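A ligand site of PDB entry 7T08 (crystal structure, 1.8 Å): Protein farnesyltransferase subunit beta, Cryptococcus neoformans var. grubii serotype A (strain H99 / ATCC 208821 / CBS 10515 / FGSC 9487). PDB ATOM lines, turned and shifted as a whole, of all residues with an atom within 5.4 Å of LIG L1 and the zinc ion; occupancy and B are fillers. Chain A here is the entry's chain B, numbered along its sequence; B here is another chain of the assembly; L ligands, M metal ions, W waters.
SG of Cys 325 sits close to OH of Tyr 409 (3.1 Å). The side-chain carboxylate (OD1) of Asp 407 is in hydrogen-bond range of the backbone NH (N) of His 410. The indole nitrogen (NE1) of Trp 329 lies within hydrogen-bond range of the side-chain hydroxyl (OH) of Tyr 409 (3.0 Å). OD1 of Asp 407 sits at hydrogen-bond distance from N of Tyr 409 (3.0 Å). The backbone carbonyl oxygen (O) of Tyr 409 sits at hydrogen-bond distance from the side-chain amide nitrogen (ND2) of Asn 413.
The guanidinium group (NH1) of Arg 197 sits at hydrogen-bond distance from a nitrogen (N5) of LIG L1 (3.3 Å). The side-chain hydroxyl (OH) of Tyr 326 lies within hydrogen-bond range of an oxygen (O7) of LG2 L2 (2.6 Å).
Merely in contact with the zinc ion: Tyr 409 (3.9 Å). Within 4 Å of the zinc ion: Asp 323, Cys 325, Tyr 409 and His 410. The nearest printed residue that does not touch the zinc ion is Asp 400 (4.3 Å).
Leu 84 touches LIG L1 (CD1 to C4, 3.9 Å). Ser 87 touches LIG L1. Trp 90 touches LIG L1. Trp 94 touches LIG L1 (CZ2 to F1, 3.4 Å). Tyr 326 touches LIG L1 (OH to C19, 3.7 Å). CH2 of Trp 329 touches F2 of LIG L1, at 3.8 Å. Asp 407 touches LIG L1 (CG to C4, 3.7 Å). Tyr 409 touches LIG L1 (CE1 to F1, 3.3 Å). Tyr 123 of chain B touches LIG L1. 13 residues have an atom within 4 Å of LIG L1: Leu 84, Ser 87, Trp 90, Trp 94, Arg 197, Asp 323, Cys 325, Tyr 326, Trp 329, Asp 407, Tyr 409, His 410 and Tyr 123 of chain B.
The zinc ion is bound by the side-chain carboxylate (OD2) of Asp 323, a ring nitrogen (NE2) of His 410, a nitrogen (N3) of LIG L1, the side-chain sulfur (SG) of Cys 325 and the side-chain carboxylate (OD1) of Asp 323. The zinc ion has five donor atoms within binding distance.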
ATOM      1  N   LEU A  84     -15.540  16.785  20.379  1.00  0.00           N
ATOM      2  CA  LEU A  84     -16.383  17.640  19.557  1.00  0.00           C
ATOM      3  C   LEU A  84     -17.768  17.043  19.321  1.00  0.00           C
ATOM      4  O   LEU A  84     -18.497  17.493  18.423  1.00  0.00           O
ATOM      5  CB  LEU A  84     -15.686  17.929  18.214  1.00  0.00           C
ATOM      6  CG  LEU A  84     -14.446  18.825  18.332  1.00  0.00           C
ATOM      7  CD1 LEU A  84     -13.552  18.690  17.102  1.00  0.00           C
ATOM      8  CD2 LEU A  84     -14.857  20.266  18.537  1.00  0.00           C
ATOM      9  N   SER A  87     -20.528  19.375  19.040  1.00  0.00           N
ATOM     10  CA  SER A  87     -20.310  20.409  18.056  1.00  0.00           C
ATOM     11  C   SER A  87     -20.323  19.826  16.642  1.00  0.00           C
ATOM     12  O   SER A  87     -19.633  20.319  15.751  1.00  0.00           O
ATOM     13  CB  SER A  87     -18.976  21.131  18.297  1.00  0.00           C
ATOM     14  OG  SER A  87     -19.068  21.997  19.424  1.00  0.00           O
ATOM     15  N   TRP A  90     -20.592  22.087  13.650  1.00  0.00           N
ATOM     16  CA  TRP A  90     -19.354  22.798  13.308  1.00  0.00           C
ATOM     17  C   TRP A  90     -18.443  21.925  12.438  1.00  0.00           C
ATOM     18  O   TRP A  90     -17.795  22.433  11.515  1.00  0.00           O
ATOM     19  CB  TRP A  90     -18.612  23.211  14.584  1.00  0.00           C
ATOM     20  CG  TRP A  90     -19.307  24.332  15.288  1.00  0.00           C
ATOM     21  CD1 TRP A  90     -20.059  24.251  16.439  1.00  0.00           C
ATOM     22  CD2 TRP A  90     -19.346  25.703  14.879  1.00  0.00           C
ATOM     23  NE1 TRP A  90     -20.552  25.496  16.770  1.00  0.00           N
ATOM     24  CE2 TRP A  90     -20.129  26.404  15.824  1.00  0.00           C
ATOM     25  CE3 TRP A  90     -18.799  26.413  13.803  1.00  0.00           C
ATOM     26  CZ2 TRP A  90     -20.372  27.775  15.736  1.00  0.00           C
ATOM     27  CZ3 TRP A  90     -19.041  27.772  13.719  1.00  0.00           C
ATOM     28  CH2 TRP A  90     -19.822  28.445  14.673  1.00  0.00           C
ATOM     29  N   TRP A  94     -17.304  23.543   8.974  1.00  0.00           N
ATOM     30  CA  TRP A  94     -15.882  23.661   8.650  1.00  0.00           C
ATOM     31  C   TRP A  94     -15.558  22.899   7.373  1.00  0.00           C
ATOM     32  O   TRP A  94     -14.777  23.366   6.536  1.00  0.00           O
ATOM     33  CB  TRP A  94     -15.013  23.144   9.801  1.00  0.00           C
ATOM     34  CG  TRP A  94     -15.105  23.992  11.093  1.00  0.00           C
ATOM     35  CD1 TRP A  94     -15.335  25.336  11.185  1.00  0.00           C
ATOM     36  CD2 TRP A  94     -14.984  23.512  12.434  1.00  0.00           C
ATOM     37  NE1 TRP A  94     -15.354  25.719  12.523  1.00  0.00           N
ATOM     38  CE2 TRP A  94     -15.134  24.613  13.295  1.00  0.00           C
ATOM     39  CE3 TRP A  94     -14.750  22.243  12.985  1.00  0.00           C
ATOM     40  CZ2 TRP A  94     -15.078  24.493  14.701  1.00  0.00           C
ATOM     41  CZ3 TRP A  94     -14.685  22.125  14.370  1.00  0.00           C
ATOM     42  CH2 TRP A  94     -14.850  23.248  15.212  1.00  0.00           C
ATOM     43  N   LEU A 141     -24.946  28.244  19.009  1.00  0.00           N
ATOM     44  CA  LEU A 141     -23.776  28.134  18.139  1.00  0.00           C
ATOM     45  C   LEU A 141     -23.981  27.055  17.081  1.00  0.00           C
ATOM     46  O   LEU A 141     -23.727  27.314  15.898  1.00  0.00           O
ATOM     47  CB  LEU A 141     -22.516  27.898  18.978  1.00  0.00           C
ATOM     48  CG  LEU A 141     -21.722  29.142  19.397  1.00  0.00           C
ATOM     49  CD1 LEU A 141     -22.594  30.102  20.203  1.00  0.00           C
ATOM     50  CD2 LEU A 141     -20.482  28.742  20.202  1.00  0.00           C
ATOM     51  N   ARG A 197     -20.493  35.634  21.365  1.00  0.00           N
ATOM     52  CA  ARG A 197     -20.634  34.535  20.408  1.00  0.00           C
ATOM     53  C   ARG A 197     -22.097  34.196  20.204  1.00  0.00           C
ATOM     54  O   ARG A 197     -22.546  33.962  19.071  1.00  0.00           O
ATOM     55  CB  ARG A 197     -19.876  33.268  20.875  1.00  0.00           C
ATOM     56  CG  ARG A 197     -18.333  33.375  20.995  1.00  0.00           C
ATOM     57  CD  ARG A 197     -17.753  32.156  21.739  1.00  0.00           C
ATOM     58  NE  ARG A 197     -18.505  31.923  22.992  1.00  0.00           N
ATOM     59  CZ  ARG A 197     -18.835  30.717  23.454  1.00  0.00           C
ATOM     60  NH1 ARG A 197     -18.456  29.610  22.807  1.00  0.00           N
ATOM     61  NH2 ARG A 197     -19.572  30.611  24.551  1.00  0.00           N
ATOM     62  N   ASP A 323      -1.412  32.969  15.019  1.00  0.00           N
ATOM     63  CA  ASP A 323      -2.134  31.711  14.827  1.00  0.00           C
ATOM     64  C   ASP A 323      -2.999  31.860  13.584  1.00  0.00           C
ATOM     65  O   ASP A 323      -3.721  32.858  13.443  1.00  0.00           O
ATOM     66  CB  ASP A 323      -2.984  31.391  16.094  1.00  0.00           C
ATOM     67  CG  ASP A 323      -3.939  30.201  15.921  1.00  0.00           C
ATOM     68  OD1 ASP A 323      -4.172  29.715  14.784  1.00  0.00           O
ATOM     69  OD2 ASP A 323      -4.490  29.750  16.945  1.00  0.00           O
ATOM     70  N   GLY A 324      -2.907  30.876  12.665  1.00  0.00           N
ATOM     71  CA  GLY A 324      -3.591  30.984  11.387  1.00  0.00           C
ATOM     72  C   GLY A 324      -5.101  31.197  11.474  1.00  0.00           C
ATOM     73  O   GLY A 324      -5.694  31.782  10.563  1.00  0.00           O
ATOM     74  N   CYS A 325      -5.756  30.693  12.522  1.00  0.00           N
ATOM     75  CA  CYS A 325      -7.218  30.876  12.531  1.00  0.00           C
ATOM     76  C   CYS A 325      -7.619  32.339  12.687  1.00  0.00           C
ATOM     77  O   CYS A 325      -8.730  32.706  12.262  1.00  0.00           O
ATOM     78  CB  CYS A 325      -7.892  30.026  13.624  1.00  0.00           C
ATOM     79  SG  CYS A 325      -7.493  30.454  15.366  1.00  0.00           S
ATOM     80  N   TYR A 326      -6.755  33.190  13.234  1.00  0.00           N
ATOM     81  CA  TYR A 326      -7.081  34.606  13.342  1.00  0.00           C
ATOM     82  C   TYR A 326      -6.990  35.334  12.015  1.00  0.00           C
ATOM     83  O   TYR A 326      -7.343  36.525  11.949  1.00  0.00           O
ATOM     84  CB  TYR A 326      -6.184  35.273  14.420  1.00  0.00           C
ATOM     85  CG  TYR A 326      -6.391  34.597  15.777  1.00  0.00           C
ATOM     86  CD1 TYR A 326      -7.675  34.413  16.292  1.00  0.00           C
ATOM     87  CD2 TYR A 326      -5.320  34.114  16.511  1.00  0.00           C
ATOM     88  CE1 TYR A 326      -7.884  33.762  17.503  1.00  0.00           C
ATOM     89  CE2 TYR A 326      -5.512  33.469  17.755  1.00  0.00           C
ATOM     90  CZ  TYR A 326      -6.807  33.300  18.231  1.00  0.00           C
ATOM     91  OH  TYR A 326      -7.033  32.675  19.431  1.00  0.00           O
ATOM     92  N   TRP A 329     -10.721  35.530  12.068  1.00  0.00           N
ATOM     93  CA  TRP A 329     -11.344  36.258  13.165  1.00  0.00           C
ATOM     94  C   TRP A 329     -10.887  37.711  13.203  1.00  0.00           C
ATOM     95  O   TRP A 329     -11.700  38.619  13.418  1.00  0.00           O
ATOM     96  CB  TRP A 329     -11.084  35.570  14.519  1.00  0.00           C
ATOM     97  CG  TRP A 329     -11.576  34.152  14.571  1.00  0.00           C
ATOM     98  CD1 TRP A 329     -10.804  33.022  14.730  1.00  0.00           C
ATOM     99  CD2 TRP A 329     -12.930  33.692  14.422  1.00  0.00           C
ATOM    100  NE1 TRP A 329     -11.608  31.892  14.696  1.00  0.00           N
ATOM    101  CE2 TRP A 329     -12.912  32.286  14.511  1.00  0.00           C
ATOM    102  CE3 TRP A 329     -14.157  34.350  14.225  1.00  0.00           C
ATOM    103  CZ2 TRP A 329     -14.081  31.505  14.408  1.00  0.00           C
ATOM    104  CZ3 TRP A 329     -15.327  33.573  14.131  1.00  0.00           C
ATOM    105  CH2 TRP A 329     -15.273  32.174  14.212  1.00  0.00           C
ATOM    106  N   ASP A 400      -2.647  25.817  13.117  1.00  0.00           N
ATOM    107  CA  ASP A 400      -2.364  27.013  13.903  1.00  0.00           C
ATOM    108  C   ASP A 400      -0.995  27.596  13.547  1.00  0.00           C
ATOM    109  O   ASP A 400      -0.894  28.743  13.082  1.00  0.00           O
ATOM    110  CB  ASP A 400      -2.476  26.616  15.396  1.00  0.00           C
ATOM    111  CG  ASP A 400      -1.735  27.527  16.372  1.00  0.00           C
ATOM    112  OD1 ASP A 400      -1.275  28.633  16.025  1.00  0.00           O
ATOM    113  OD2 ASP A 400      -1.618  27.109  17.543  1.00  0.00           O
ATOM    114  N   ASP A 407      -6.286  20.651  11.638  1.00  0.00           N
ATOM    115  CA  ASP A 407      -7.626  20.223  12.022  1.00  0.00           C
ATOM    116  C   ASP A 407      -8.640  20.966  11.180  1.00  0.00           C
ATOM    117  O   ASP A 407      -8.310  21.920  10.461  1.00  0.00           O
ATOM    118  CB  ASP A 407      -7.871  20.434  13.532  1.00  0.00           C
ATOM    119  CG  ASP A 407      -7.748  21.891  13.956  1.00  0.00           C
ATOM    120  OD1 ASP A 407      -8.484  22.741  13.426  1.00  0.00           O
ATOM    121  OD2 ASP A 407      -6.924  22.185  14.858  1.00  0.00           O
ATOM    122  N   GLN A 408      -9.896  20.522  11.253  1.00  0.00           N
ATOM    123  CA  GLN A 408     -10.931  21.095  10.399  1.00  0.00           C
ATOM    124  C   GLN A 408     -11.200  22.562  10.733  1.00  0.00           C
ATOM    125  O   GLN A 408     -11.520  23.355   9.835  1.00  0.00           O
ATOM    126  CB  GLN A 408     -12.229  20.299  10.527  1.00  0.00           C
ATOM    127  CG  GLN A 408     -12.129  18.857  10.002  1.00  0.00           C
ATOM    128  CD  GLN A 408     -11.567  17.898  11.031  1.00  0.00           C
ATOM    129  OE1 GLN A 408     -11.058  18.306  12.085  1.00  0.00           O
ATOM    130  NE2 GLN A 408     -11.666  16.607  10.736  1.00  0.00           N
ATOM    131  N   TYR A 409     -11.076  22.943  12.006  1.00  0.00           N
ATOM    132  CA  TYR A 409     -11.342  24.315  12.413  1.00  0.00           C
ATOM    133  C   TYR A 409     -10.283  25.266  11.851  1.00  0.00           C
ATOM    134  O   TYR A 409     -10.613  26.347  11.346  1.00  0.00           O
ATOM    135  CB  TYR A 409     -11.415  24.386  13.950  1.00  0.00           C
ATOM    136  CG  TYR A 409     -11.177  25.764  14.533  1.00  0.00           C
ATOM    137  CD1 TYR A 409     -12.238  26.669  14.736  1.00  0.00           C
ATOM    138  CD2 TYR A 409      -9.889  26.176  14.890  1.00  0.00           C
ATOM    139  CE1 TYR A 409     -12.005  27.950  15.275  1.00  0.00           C
ATOM    140  CE2 TYR A 409      -9.647  27.448  15.423  1.00  0.00           C
ATOM    141  CZ  TYR A 409     -10.695  28.324  15.605  1.00  0.00           C
ATOM    142  OH  TYR A 409     -10.420  29.577  16.117  1.00  0.00           O
ATOM    143  N   HIS A 410      -8.999  24.892  11.922  1.00  0.00           N
ATOM    144  CA  HIS A 410      -7.961  25.736  11.338  1.00  0.00           C
ATOM    145  C   HIS A 410      -7.978  25.691   9.812  1.00  0.00           C
ATOM    146  O   HIS A 410      -7.540  26.647   9.160  1.00  0.00           O
ATOM    147  CB  HIS A 410      -6.579  25.348  11.873  1.00  0.00           C
ATOM    148  CG  HIS A 410      -6.345  25.834  13.276  1.00  0.00           C
ATOM    149  ND1 HIS A 410      -6.473  25.011  14.374  1.00  0.00           N
ATOM    150  CD2 HIS A 410      -6.064  27.061  13.755  1.00  0.00           C
ATOM    151  CE1 HIS A 410      -6.241  25.716  15.472  1.00  0.00           C
ATOM    152  NE2 HIS A 410      -6.014  26.968  15.129  1.00  0.00           N
ATOM    153  N   ASN A 413     -10.789  28.269   8.967  1.00  0.00           N
ATOM    154  CA  ASN A 413     -10.540  29.676   9.277  1.00  0.00           C
ATOM    155  C   ASN A 413      -9.284  30.222   8.598  1.00  0.00           C
ATOM    156  O   ASN A 413      -9.276  31.404   8.236  1.00  0.00           O
ATOM    157  CB  ASN A 413     -10.506  29.868  10.811  1.00  0.00           C
ATOM    158  CG  ASN A 413     -11.907  29.825  11.400  1.00  0.00           C
ATOM    159  OD1 ASN A 413     -12.736  30.665  11.084  1.00  0.00           O
ATOM    160  ND2 ASN A 413     -12.193  28.795  12.194  1.00  0.00           N
ATOM    161  N   TYR B 123     -15.724  25.732  28.138  1.00  0.00           N
ATOM    162  CA  TYR B 123     -16.691  26.766  28.524  1.00  0.00           C
ATOM    163  C   TYR B 123     -17.714  26.217  29.512  1.00  0.00           C
ATOM    164  O   TYR B 123     -18.173  26.938  30.412  1.00  0.00           O
ATOM    165  CB  TYR B 123     -17.449  27.308  27.307  1.00  0.00           C
ATOM    166  CG  TYR B 123     -16.753  28.332  26.435  1.00  0.00           C
ATOM    167  CD1 TYR B 123     -16.889  29.709  26.690  1.00  0.00           C
ATOM    168  CD2 TYR B 123     -16.033  27.942  25.317  1.00  0.00           C
ATOM    169  CE1 TYR B 123     -16.294  30.651  25.842  1.00  0.00           C
ATOM    170  CE2 TYR B 123     -15.424  28.875  24.485  1.00  0.00           C
ATOM    171  CZ  TYR B 123     -15.570  30.221  24.737  1.00  0.00           C
ATOM    172  OH  TYR B 123     -14.977  31.135  23.877  1.00  0.00           O
HETATM  173  C1  LIG L   1     -16.417  24.225  18.863  1.00  0.00           C
HETATM  174  C2  LIG L   1     -11.044  25.656  21.188  1.00  0.00           C
HETATM  175  C3  LIG L   1      -8.243  27.238  19.585  1.00  0.00           C
HETATM  176  C4  LIG L   1     -10.663  21.113  16.151  1.00  0.00           C
HETATM  177  C5  LIG L   1     -10.417  21.746  17.540  1.00  0.00           C
HETATM  178  C6  LIG L   1     -10.494  23.282  17.518  1.00  0.00           C
HETATM  179  C7  LIG L   1     -10.366  23.906  18.956  1.00  0.00           C
HETATM  180  C8  LIG L   1     -10.507  25.518  18.910  1.00  0.00           C
HETATM  181  C9  LIG L   1     -11.897  25.828  18.411  1.00  0.00           C
HETATM  182  C10 LIG L   1     -14.387  25.490  19.005  1.00  0.00           C
HETATM  183  C11 LIG L   1     -15.090  24.325  19.285  1.00  0.00           C
HETATM  184  C12 LIG L   1     -17.008  25.264  18.166  1.00  0.00           C
HETATM  185  C13 LIG L   1     -16.296  26.430  17.866  1.00  0.00           C
HETATM  186  C14 LIG L   1     -16.182  28.395  16.448  1.00  0.00           C
HETATM  187  C15 LIG L   1     -14.971  26.533  18.297  1.00  0.00           C
HETATM  188  C16 LIG L   1     -12.588  25.518  20.843  1.00  0.00           C
HETATM  189  C17 LIG L   1      -8.990  26.197  20.486  1.00  0.00           C
HETATM  190  C18 LIG L   1      -7.503  26.945  18.438  1.00  0.00           C
HETATM  191  C19 LIG L   1      -7.460  29.099  18.751  1.00  0.00           C
HETATM  192  C20 LIG L   1      -8.787  29.364  20.832  1.00  0.00           C
HETATM  193  C21 LIG L   1     -10.347  29.330  20.866  1.00  0.00           C
HETATM  194  C22 LIG L   1     -11.015  29.268  22.075  1.00  0.00           C
HETATM  195  C23 LIG L   1     -12.412  29.254  22.104  1.00  0.00           C
HETATM  196  C24 LIG L   1     -13.126  29.310  20.902  1.00  0.00           C
HETATM  197  C25 LIG L   1     -14.655  29.294  20.892  1.00  0.00           C
HETATM  198  C26 LIG L   1     -12.446  29.377  19.704  1.00  0.00           C
HETATM  199  C27 LIG L   1     -11.063  29.389  19.673  1.00  0.00           C
HETATM  200  F1  LIG L   1     -15.247  27.764  15.692  1.00  0.00           F
HETATM  201  F2  LIG L   1     -17.024  29.108  15.650  1.00  0.00           F
HETATM  202  F3  LIG L   1     -15.526  29.267  17.265  1.00  0.00           F
HETATM  203  F4  LIG L   1     -13.141  29.425  18.539  1.00  0.00           F
HETATM  204  N1  LIG L   1     -12.964  25.615  19.432  1.00  0.00           N
HETATM  205  N2  LIG L   1     -10.260  26.146  20.153  1.00  0.00           N
HETATM  206  N3  LIG L   1      -7.029  28.104  17.958  1.00  0.00           N
HETATM  207  N4  LIG L   1      -8.184  28.573  19.732  1.00  0.00           N
HETATM  208  N5  LIG L   1     -15.797  29.288  20.859  1.00  0.00           N
HETATM  209  O1  LIG L   1     -16.943  27.462  17.163  1.00  0.00           O
HETATM  210  O2  LIG L   1     -13.412  25.341  21.686  1.00  0.00           O
HETATM  211  C1  LG2 L   2      -8.722  32.143  24.034  1.00  0.00           C
HETATM  212  O1  LG2 L   2      -8.208  30.853  23.762  1.00  0.00           O
HETATM  213  C2  LG2 L   2      -9.938  32.422  23.133  1.00  0.00           C
HETATM  214  C3  LG2 L   2     -11.205  32.482  23.549  1.00  0.00           C
HETATM  215  C4  LG2 L   2     -11.595  32.267  25.028  1.00  0.00           C
HETATM  216  C5  LG2 L   2     -12.348  32.762  22.564  1.00  0.00           C
HETATM  217  C6  LG2 L   2     -11.931  32.820  21.076  1.00  0.00           C
HETATM  218  C7  LG2 L   2     -13.193  32.822  20.186  1.00  0.00           C
HETATM  219  C8  LG2 L   2     -13.112  32.628  18.859  1.00  0.00           C
HETATM  220  C9  LG2 L   2     -11.752  32.435  18.182  1.00  0.00           C
HETATM  221  C10 LG2 L   2     -14.324  32.616  17.917  1.00  0.00           C
HETATM  222  C11 LG2 L   2     -15.723  32.634  18.550  1.00  0.00           C
HETATM  223  C12 LG2 L   2     -16.764  32.837  17.424  1.00  0.00           C
HETATM  224  C13 LG2 L   2     -17.862  32.084  17.227  1.00  0.00           C
HETATM  225  C14 LG2 L   2     -18.809  32.427  16.068  1.00  0.00           C
HETATM  226  C15 LG2 L   2     -18.227  30.905  18.132  1.00  0.00           C
HETATM  227  P1  LG2 L   2      -6.587  30.537  23.830  1.00  0.00           P
HETATM  228  O2  LG2 L   2      -5.945  31.096  25.076  1.00  0.00           O
HETATM  229  O3  LG2 L   2      -6.429  29.047  23.700  1.00  0.00           O
HETATM  230  O4  LG2 L   2      -5.887  31.199  22.504  1.00  0.00           O
HETATM  231  P2  LG2 L   2      -4.995  32.566  22.377  1.00  0.00           P
HETATM  232  O5  LG2 L   2      -3.672  32.296  23.056  1.00  0.00           O
HETATM  233  O6  LG2 L   2      -5.735  33.730  22.976  1.00  0.00           O
HETATM  234  O7  LG2 L   2      -4.816  32.716  20.868  1.00  0.00           O
HETATM  235 ZN    ZN M   1      -6.104  28.763  16.188  1.00  0.00          ZN
HETATM  236  O   HOH W   1      -5.102  28.268  21.319  1.00  0.00           O
